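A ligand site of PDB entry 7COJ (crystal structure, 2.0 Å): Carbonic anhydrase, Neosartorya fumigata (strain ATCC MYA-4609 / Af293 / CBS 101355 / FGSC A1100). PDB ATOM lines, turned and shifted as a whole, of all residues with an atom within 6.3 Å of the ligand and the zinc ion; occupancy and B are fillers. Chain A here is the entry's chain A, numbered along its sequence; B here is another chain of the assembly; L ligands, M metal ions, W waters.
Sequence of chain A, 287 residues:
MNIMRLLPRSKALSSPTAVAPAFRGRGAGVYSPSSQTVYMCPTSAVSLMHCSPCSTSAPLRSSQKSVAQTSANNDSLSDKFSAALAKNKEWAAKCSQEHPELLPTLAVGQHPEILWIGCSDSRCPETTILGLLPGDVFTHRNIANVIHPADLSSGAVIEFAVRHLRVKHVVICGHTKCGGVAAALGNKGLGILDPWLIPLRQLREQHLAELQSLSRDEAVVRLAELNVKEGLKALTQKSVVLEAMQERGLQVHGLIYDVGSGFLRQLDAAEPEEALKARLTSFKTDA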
ATOM      1  N   CYS A 119      23.782  18.688  -5.886  1.00  0.00           N
ATOM      2  CA  CYS A 119      24.814  19.663  -5.539  1.00  0.00           C
ATOM      3  C   CYS A 119      25.684  19.933  -6.774  1.00  0.00           C
ATOM      4  O   CYS A 119      25.936  19.005  -7.574  1.00  0.00           O
ATOM      5  CB  CYS A 119      25.613  19.218  -4.330  1.00  0.00           C
ATOM      6  SG  CYS A 119      26.644  20.532  -3.789  1.00  0.00           S
ATOM      7  N   SER A 120      26.178  21.153  -6.877  1.00  0.00           N
ATOM      8  CA  SER A 120      27.184  21.596  -7.891  1.00  0.00           C
ATOM      9  C   SER A 120      28.502  20.875  -7.675  1.00  0.00           C
ATOM     10  O   SER A 120      29.358  20.880  -8.577  1.00  0.00           O
ATOM     11  CB  SER A 120      27.329  23.077  -7.799  1.00  0.00           C
ATOM     12  OG  SER A 120      26.128  23.705  -8.208  1.00  0.00           O
ATOM     13  N   ASP A 121      28.731  20.316  -6.479  1.00  0.00           N
ATOM     14  CA  ASP A 121      29.993  19.632  -6.121  1.00  0.00           C
ATOM     15  C   ASP A 121      30.458  18.793  -7.323  1.00  0.00           C
ATOM     16  O   ASP A 121      29.669  17.979  -7.866  1.00  0.00           O
ATOM     17  CB  ASP A 121      29.814  18.752  -4.854  1.00  0.00           C
ATOM     18  CG  ASP A 121      31.102  18.226  -4.274  1.00  0.00           C
ATOM     19  OD1 ASP A 121      31.818  17.425  -4.966  1.00  0.00           O
ATOM     20  OD2 ASP A 121      31.368  18.578  -3.132  1.00  0.00           O
ATOM     21  N   SER A 122      31.729  18.974  -7.718  1.00  0.00           N
ATOM     22  CA  SER A 122      32.335  18.355  -8.914  1.00  0.00           C
ATOM     23  C   SER A 122      32.290  16.832  -8.800  1.00  0.00           C
ATOM     24  O   SER A 122      32.369  16.177  -9.856  1.00  0.00           O
ATOM     25  CB  SER A 122      33.725  18.833  -9.112  1.00  0.00           C
ATOM     26  OG  SER A 122      34.568  18.454  -8.020  1.00  0.00           O
ATOM     27  N   ARG A 123      32.189  16.295  -7.593  1.00  0.00           N
ATOM     28  CA  ARG A 123      32.181  14.836  -7.375  1.00  0.00           C
ATOM     29  C   ARG A 123      30.791  14.225  -7.624  1.00  0.00           C
ATOM     30  O   ARG A 123      30.735  12.993  -7.573  1.00  0.00           O
ATOM     31  CB  ARG A 123      32.683  14.503  -5.963  1.00  0.00           C
ATOM     32  CG  ARG A 123      34.089  15.035  -5.710  1.00  0.00           C
ATOM     33  CD  ARG A 123      34.532  15.028  -4.256  1.00  0.00           C
ATOM     34  NE  ARG A 123      33.776  15.976  -3.482  1.00  0.00           N
ATOM     35  CZ  ARG A 123      33.871  16.152  -2.167  1.00  0.00           C
ATOM     36  NH1 ARG A 123      34.824  15.532  -1.466  1.00  0.00           N
ATOM     37  NH2 ARG A 123      33.097  17.055  -1.566  1.00  0.00           N
ATOM     38  N   CYS A 124      29.726  14.990  -7.935  1.00  0.00           N
ATOM     39  CA  CYS A 124      28.338  14.467  -8.113  1.00  0.00           C
ATOM     40  C   CYS A 124      27.779  14.718  -9.512  1.00  0.00           C
ATOM     41  O   CYS A 124      26.677  15.258  -9.646  1.00  0.00           O
ATOM     42  CB  CYS A 124      27.423  15.108  -7.085  1.00  0.00           C
ATOM     43  SG  CYS A 124      28.078  15.048  -5.392  1.00  0.00           S
ATOM     44  N   ASN A 142      23.044  23.112  -7.758  1.00  0.00           N
ATOM     45  CA  ASN A 142      23.277  24.388  -7.060  1.00  0.00           C
ATOM     46  C   ASN A 142      24.074  24.053  -5.806  1.00  0.00           C
ATOM     47  O   ASN A 142      24.303  22.848  -5.539  1.00  0.00           O
ATOM     48  CB  ASN A 142      21.967  25.161  -6.880  1.00  0.00           C
ATOM     49  CG  ASN A 142      21.013  24.506  -5.899  1.00  0.00           C
ATOM     50  OD1 ASN A 142      21.472  23.774  -5.021  1.00  0.00           O
ATOM     51  ND2 ASN A 142      19.718  24.819  -6.024  1.00  0.00           N
ATOM     52  N   ILE A 143      24.513  25.063  -5.059  1.00  0.00           N
ATOM     53  CA  ILE A 143      25.300  24.818  -3.825  1.00  0.00           C
ATOM     54  C   ILE A 143      24.394  24.100  -2.819  1.00  0.00           C
ATOM     55  O   ILE A 143      23.382  24.706  -2.382  1.00  0.00           O
ATOM     56  CB  ILE A 143      25.839  26.131  -3.233  1.00  0.00           C
ATOM     57  CG1 ILE A 143      26.787  26.872  -4.197  1.00  0.00           C
ATOM     58  CG2 ILE A 143      26.497  25.870  -1.892  1.00  0.00           C
ATOM     59  CD1 ILE A 143      28.014  26.098  -4.506  1.00  0.00           C
ATOM     60  N   ALA A 144      24.773  22.883  -2.433  1.00  0.00           N
ATOM     61  CA  ALA A 144      24.132  22.083  -1.375  1.00  0.00           C
ATOM     62  C   ALA A 144      22.693  21.699  -1.742  1.00  0.00           C
ATOM     63  O   ALA A 144      21.914  21.358  -0.819  1.00  0.00           O
ATOM     64  CB  ALA A 144      24.185  22.822  -0.069  1.00  0.00           C
ATOM     65  N   ASN A 145      22.367  21.631  -3.030  1.00  0.00           N
ATOM     66  CA  ASN A 145      21.055  21.103  -3.496  1.00  0.00           C
ATOM     67  C   ASN A 145      19.947  21.715  -2.641  1.00  0.00           C
ATOM     68  O   ASN A 145      19.053  20.990  -2.207  1.00  0.00           O
ATOM     69  CB  ASN A 145      21.018  19.559  -3.504  1.00  0.00           C
ATOM     70  CG  ASN A 145      21.516  18.877  -2.245  1.00  0.00           C
ATOM     71  OD1 ASN A 145      22.723  18.658  -2.077  1.00  0.00           O
ATOM     72  ND2 ASN A 145      20.576  18.514  -1.356  1.00  0.00           N
ATOM     73  N   HIS A 175      24.763  14.858  -0.612  1.00  0.00           N
ATOM     74  CA  HIS A 175      25.969  13.992  -0.678  1.00  0.00           C
ATOM     75  C   HIS A 175      26.750  14.116   0.632  1.00  0.00           C
ATOM     76  O   HIS A 175      26.549  15.098   1.372  1.00  0.00           O
ATOM     77  CB  HIS A 175      26.792  14.293  -1.947  1.00  0.00           C
ATOM     78  CG  HIS A 175      27.451  15.615  -1.878  1.00  0.00           C
ATOM     79  ND1 HIS A 175      28.803  15.758  -1.548  1.00  0.00           N
ATOM     80  CD2 HIS A 175      26.960  16.852  -2.091  1.00  0.00           C
ATOM     81  CE1 HIS A 175      29.107  17.046  -1.550  1.00  0.00           C
ATOM     82  NE2 HIS A 175      28.015  17.690  -1.912  1.00  0.00           N
ATOM     83  N   LYS A 177      30.162  14.722   2.776  1.00  0.00           N
ATOM     84  CA  LYS A 177      31.273  15.706   2.660  1.00  0.00           C
ATOM     85  C   LYS A 177      30.789  16.927   1.842  1.00  0.00           C
ATOM     86  O   LYS A 177      31.574  17.462   1.072  1.00  0.00           O
ATOM     87  CB  LYS A 177      32.471  15.032   1.995  1.00  0.00           C
ATOM     88  CG  LYS A 177      32.897  13.701   2.611  1.00  0.00           C
ATOM     89  CD  LYS A 177      33.429  13.884   3.983  1.00  0.00           C
ATOM     90  CE  LYS A 177      34.884  14.294   3.938  1.00  0.00           C
ATOM     91  NZ  LYS A 177      35.262  15.277   4.981  1.00  0.00           N
ATOM     92  N   CYS A 178      29.518  17.301   1.964  1.00  0.00           N
ATOM     93  CA  CYS A 178      28.982  18.537   1.336  1.00  0.00           C
ATOM     94  C   CYS A 178      29.482  19.722   2.156  1.00  0.00           C
ATOM     95  O   CYS A 178      28.997  19.915   3.279  1.00  0.00           O
ATOM     96  CB  CYS A 178      27.460  18.507   1.182  1.00  0.00           C
ATOM     97  SG  CYS A 178      26.823  19.959   0.362  1.00  0.00           S
ATOM     98  N   GLY A 179      30.413  20.496   1.579  1.00  0.00           N
ATOM     99  CA  GLY A 179      30.977  21.658   2.282  1.00  0.00           C
ATOM    100  C   GLY A 179      29.964  22.787   2.412  1.00  0.00           C
ATOM    101  O   GLY A 179      30.143  23.615   3.285  1.00  0.00           O
ATOM    102  N   GLY A 180      28.938  22.841   1.542  1.00  0.00           N
ATOM    103  CA  GLY A 180      27.816  23.771   1.729  1.00  0.00           C
ATOM    104  C   GLY A 180      27.081  23.504   3.037  1.00  0.00           C
ATOM    105  O   GLY A 180      26.848  24.455   3.834  1.00  0.00           O
ATOM    106  N   VAL A 181      26.712  22.256   3.267  1.00  0.00           N
ATOM    107  CA  VAL A 181      26.073  21.818   4.548  1.00  0.00           C
ATOM    108  C   VAL A 181      27.032  22.134   5.709  1.00  0.00           C
ATOM    109  O   VAL A 181      26.590  22.708   6.709  1.00  0.00           O
ATOM    110  CB  VAL A 181      25.699  20.322   4.465  1.00  0.00           C
ATOM    111  CG1 VAL A 181      25.239  19.787   5.820  1.00  0.00           C
ATOM    112  CG2 VAL A 181      24.630  20.092   3.395  1.00  0.00           C
ATOM    113  N   ALA A 183      29.430  24.392   5.888  1.00  0.00           N
ATOM    114  CA  ALA A 183      29.513  25.864   6.065  1.00  0.00           C
ATOM    115  C   ALA A 183      28.320  26.351   6.896  1.00  0.00           C
ATOM    116  O   ALA A 183      28.513  27.251   7.708  1.00  0.00           O
ATOM    117  CB  ALA A 183      29.577  26.558   4.724  1.00  0.00           C
ATOM    118  N   LYS A 188      31.216  31.484  10.120  1.00  0.00           N
ATOM    119  CA  LYS A 188      32.108  32.373   9.319  1.00  0.00           C
ATOM    120  C   LYS A 188      31.206  33.097   8.305  1.00  0.00           C
ATOM    121  O   LYS A 188      30.338  32.420   7.700  1.00  0.00           O
ATOM    122  CB  LYS A 188      33.228  31.543   8.675  1.00  0.00           C
ATOM    123  CG  LYS A 188      33.985  30.590   9.601  1.00  0.00           C
ATOM    124  CD  LYS A 188      34.427  29.228   8.983  1.00  0.00           C
ATOM    125  CE  LYS A 188      33.361  28.126   9.014  1.00  0.00           C
ATOM    126  NZ  LYS A 188      32.416  28.171   7.868  1.00  0.00           N
ATOM    127  N   LEU A 190      30.318  34.577   4.831  1.00  0.00           N
ATOM    128  CA  LEU A 190      30.774  34.016   3.521  1.00  0.00           C
ATOM    129  C   LEU A 190      30.265  34.869   2.369  1.00  0.00           C
ATOM    130  O   LEU A 190      30.213  34.359   1.212  1.00  0.00           O
ATOM    131  CB  LEU A 190      30.292  32.573   3.448  1.00  0.00           C
ATOM    132  CG  LEU A 190      30.971  31.625   4.437  1.00  0.00           C
ATOM    133  CD1 LEU A 190      30.125  30.385   4.640  1.00  0.00           C
ATOM    134  CD2 LEU A 190      32.388  31.321   3.989  1.00  0.00           C
ATOM    135  N   LEU A 193      27.261  33.902  -0.252  1.00  0.00           N
ATOM    136  CA  LEU A 193      26.882  32.514   0.156  1.00  0.00           C
ATOM    137  C   LEU A 193      25.960  32.535   1.387  1.00  0.00           C
ATOM    138  O   LEU A 193      25.185  31.577   1.501  1.00  0.00           O
ATOM    139  CB  LEU A 193      28.156  31.692   0.415  1.00  0.00           C
ATOM    140  CG  LEU A 193      28.833  31.194  -0.864  1.00  0.00           C
ATOM    141  CD1 LEU A 193      30.296  30.877  -0.595  1.00  0.00           C
ATOM    142  CD2 LEU A 193      28.100  29.971  -1.404  1.00  0.00           C
ATOM    143  N   LEU A 197      22.629  30.043   1.911  1.00  0.00           N
ATOM    144  CA  LEU A 197      22.654  28.907   2.859  1.00  0.00           C
ATOM    145  C   LEU A 197      21.589  29.079   3.965  1.00  0.00           C
ATOM    146  O   LEU A 197      21.506  28.198   4.855  1.00  0.00           O
ATOM    147  CB  LEU A 197      24.064  28.816   3.454  1.00  0.00           C
ATOM    148  CG  LEU A 197      25.162  28.431   2.470  1.00  0.00           C
ATOM    149  CD1 LEU A 197      26.521  28.526   3.106  1.00  0.00           C
ATOM    150  CD2 LEU A 197      24.961  27.052   1.891  1.00  0.00           C
ATOM    151  N   GLN B 110      37.588  18.034  -3.125  1.00  0.00           N
ATOM    152  CA  GLN B 110      37.498  18.240  -4.576  1.00  0.00           C
ATOM    153  C   GLN B 110      38.502  19.328  -4.960  1.00  0.00           C
ATOM    154  O   GLN B 110      38.724  20.239  -4.167  1.00  0.00           O
ATOM    155  CB  GLN B 110      36.064  18.596  -4.946  1.00  0.00           C
ATOM    156  CG  GLN B 110      35.577  19.897  -4.346  1.00  0.00           C
ATOM    157  CD  GLN B 110      34.197  20.279  -4.791  1.00  0.00           C
ATOM    158  OE1 GLN B 110      33.851  20.097  -5.962  1.00  0.00           O
ATOM    159  NE2 GLN B 110      33.424  20.866  -3.886  1.00  0.00           N
ATOM    160  N   PHE B 138      33.056  21.495 -11.656  1.00  0.00           N
ATOM    161  CA  PHE B 138      32.073  22.121 -10.761  1.00  0.00           C
ATOM    162  C   PHE B 138      30.932  22.626 -11.627  1.00  0.00           C
ATOM    163  O   PHE B 138      31.213  23.295 -12.636  1.00  0.00           O
ATOM    164  CB  PHE B 138      32.715  23.209  -9.930  1.00  0.00           C
ATOM    165  CG  PHE B 138      31.899  23.551  -8.714  1.00  0.00           C
ATOM    166  CD1 PHE B 138      31.896  22.716  -7.617  1.00  0.00           C
ATOM    167  CD2 PHE B 138      31.113  24.686  -8.699  1.00  0.00           C
ATOM    168  CE1 PHE B 138      31.145  23.041  -6.501  1.00  0.00           C
ATOM    169  CE2 PHE B 138      30.385  25.025  -7.566  1.00  0.00           C
ATOM    170  CZ  PHE B 138      30.367  24.172  -6.499  1.00  0.00           C
ATOM    171  N   PHE B 160      31.651  30.639  -4.786  1.00  0.00           N
ATOM    172  CA  PHE B 160      32.308  29.434  -4.232  1.00  0.00           C
ATOM    173  C   PHE B 160      33.387  28.903  -5.181  1.00  0.00           C
ATOM    174  O   PHE B 160      34.527  28.660  -4.754  1.00  0.00           O
ATOM    175  CB  PHE B 160      31.306  28.351  -3.856  1.00  0.00           C
ATOM    176  CG  PHE B 160      32.012  27.167  -3.273  1.00  0.00           C
ATOM    177  CD1 PHE B 160      32.650  27.286  -2.040  1.00  0.00           C
ATOM    178  CD2 PHE B 160      32.138  25.976  -3.976  1.00  0.00           C
ATOM    179  CE1 PHE B 160      33.333  26.198  -1.502  1.00  0.00           C
ATOM    180  CE2 PHE B 160      32.826  24.911  -3.433  1.00  0.00           C
ATOM    181  CZ  PHE B 160      33.451  25.037  -2.201  1.00  0.00           C
ATOM    182  N   HIS B 164      36.731  30.141  -3.532  1.00  0.00           N
ATOM    183  CA  HIS B 164      37.102  29.013  -2.619  1.00  0.00           C
ATOM    184  C   HIS B 164      37.815  27.886  -3.387  1.00  0.00           C
ATOM    185  O   HIS B 164      38.899  27.497  -2.987  1.00  0.00           O
ATOM    186  CB  HIS B 164      35.886  28.519  -1.849  1.00  0.00           C
ATOM    187  CG  HIS B 164      35.253  29.572  -1.002  1.00  0.00           C
ATOM    188  ND1 HIS B 164      35.222  29.468   0.373  1.00  0.00           N
ATOM    189  CD2 HIS B 164      34.523  30.660  -1.309  1.00  0.00           C
ATOM    190  CE1 HIS B 164      34.595  30.518   0.885  1.00  0.00           C
ATOM    191  NE2 HIS B 164      34.154  31.277  -0.131  1.00  0.00           N
ATOM    192  N   LEU B 165      37.243  27.368  -4.457  1.00  0.00           N
ATOM    193  CA  LEU B 165      37.867  26.240  -5.182  1.00  0.00           C
ATOM    194  C   LEU B 165      38.998  26.765  -6.048  1.00  0.00           C
ATOM    195  O   LEU B 165      39.829  25.958  -6.418  1.00  0.00           O
ATOM    196  CB  LEU B 165      36.836  25.495  -6.026  1.00  0.00           C
ATOM    197  CG  LEU B 165      35.775  24.742  -5.220  1.00  0.00           C
ATOM    198  CD1 LEU B 165      34.836  24.018  -6.167  1.00  0.00           C
ATOM    199  CD2 LEU B 165      36.398  23.777  -4.225  1.00  0.00           C
HETATM  200  C1  LIG L   1      30.544  23.062  -1.343  1.00  0.00           C
HETATM  201  C2  LIG L   1      31.190  24.747   0.174  1.00  0.00           C
HETATM  202  C3  LIG L   1      30.634  26.964   0.958  1.00  0.00           C
HETATM  203  C4  LIG L   1      31.126  28.100   1.794  1.00  0.00           C
HETATM  204  N1  LIG L   1      29.646  20.605  -1.885  1.00  0.00           N
HETATM  205  N2  LIG L   1      31.959  23.678   0.234  1.00  0.00           N
HETATM  206  N3  LIG L   1      31.602  22.727  -0.707  1.00  0.00           N
HETATM  207  N4  LIG L   1      31.432  25.855   0.953  1.00  0.00           N
HETATM  208  O1  LIG L   1      28.546  22.664  -2.759  1.00  0.00           O
HETATM  209  O2  LIG L   1      30.776  21.911  -3.587  1.00  0.00           O
HETATM  210  O3  LIG L   1      29.615  26.996   0.288  1.00  0.00           O
HETATM  211  S1  LIG L   1      29.801  22.021  -2.564  1.00  0.00           S
HETATM  212  S2  LIG L   1      29.931  24.606  -0.966  1.00  0.00           S
HETATM  213 ZN    ZN M   1      27.700  19.801  -1.844  1.00  0.00          ZN
HETATM  214  O   HOH W   1      33.519  25.920   2.594  1.00  0.00           O
HETATM  215  O   HOH W   2      34.663  23.209   0.663  1.00  0.00           O
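Asp 121 touches the zinc ion.
Within 4 Å of the zinc ion: Cys 119, Asp 121, His 175 and Cys 178.
The side-chain carboxylate of Asp 121 is in salt-bridge range of the guanidinium group of Arg 123 (2.8 Å).
The side-chain sulfur (SG) of Cys 119 lies close to the backbone NH (N) of Ala 144 (3.3 Å).
O of Asn 142 lies close to SG of Cys 119 (3.7 Å).
N of Val 181 sits close to SG of Cys 178.
The backbone carbonyl oxygen (O) of Phe 160 of chain B lies within hydrogen-bond range of the backbone NH (N) of Leu 165 of chain B (3.0 Å).
The side-chain amide nitrogen (NE2) of Gln 110 of chain B sits at hydrogen-bond distance from the side-chain carboxylate (OD2) of Asp 121, at 3.2 Å.
The side-chain hydroxyl (OG) of Ser 122 sits at hydrogen-bond distance from the side-chain amide oxygen (OE1) of Gln 110 of chain B, at 2.7 Å.
The side-chain sulfur of Cys 178 lies close to the backbone NH of Gly 180 (3.8 Å).
Merely in contact with the ligand: Ile 143, Ala 144, Ala 183, Leu 190, Leu 193, Phe 138 of chain B and Phe 160 of chain B.
Within 4 Å of the ligand: Cys 119, Asp 121, Ile 143, Ala 144, His 175, Cys 178, Gly 179, Gly 180, Ala 183, Leu 190, Leu 193, Gln 110 of chain B, Phe 138 of chain B and Phe 160 of chain B.
Along chain A the residues within 4 Å of the ligand span positions 119 to 193.
The nearest printed residue that does not touch the ligand is His 164 of chain B (4.3 Å).
N1 of the ligand lies close to OD2 of Asp 121.
A sulfur (S2) of the ligand sits close to the backbone NH of Gly 180.
The backbone NH (N) of Gly 179 sits close to a nitrogen (N3) of the ligand, 3.4 Å away.
O of Gly 179 sits close to N4 of the ligand (3.5 Å).
The side-chain amide nitrogen of Gln 110 of chain B sits at hydrogen-bond distance from an oxygen (O2) of the ligand (2.9 Å).
A nitrogen (N1) of the ligand binds the zinc ion, 2.1 Å away.
NE2 of His 175 binds the zinc ion (2.1 Å).
SG of Cys 119 is bound to the zinc ion (2.3 Å).
The zinc ion is bound by the side-chain sulfur (SG) of Cys 178 (2.4 Å).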
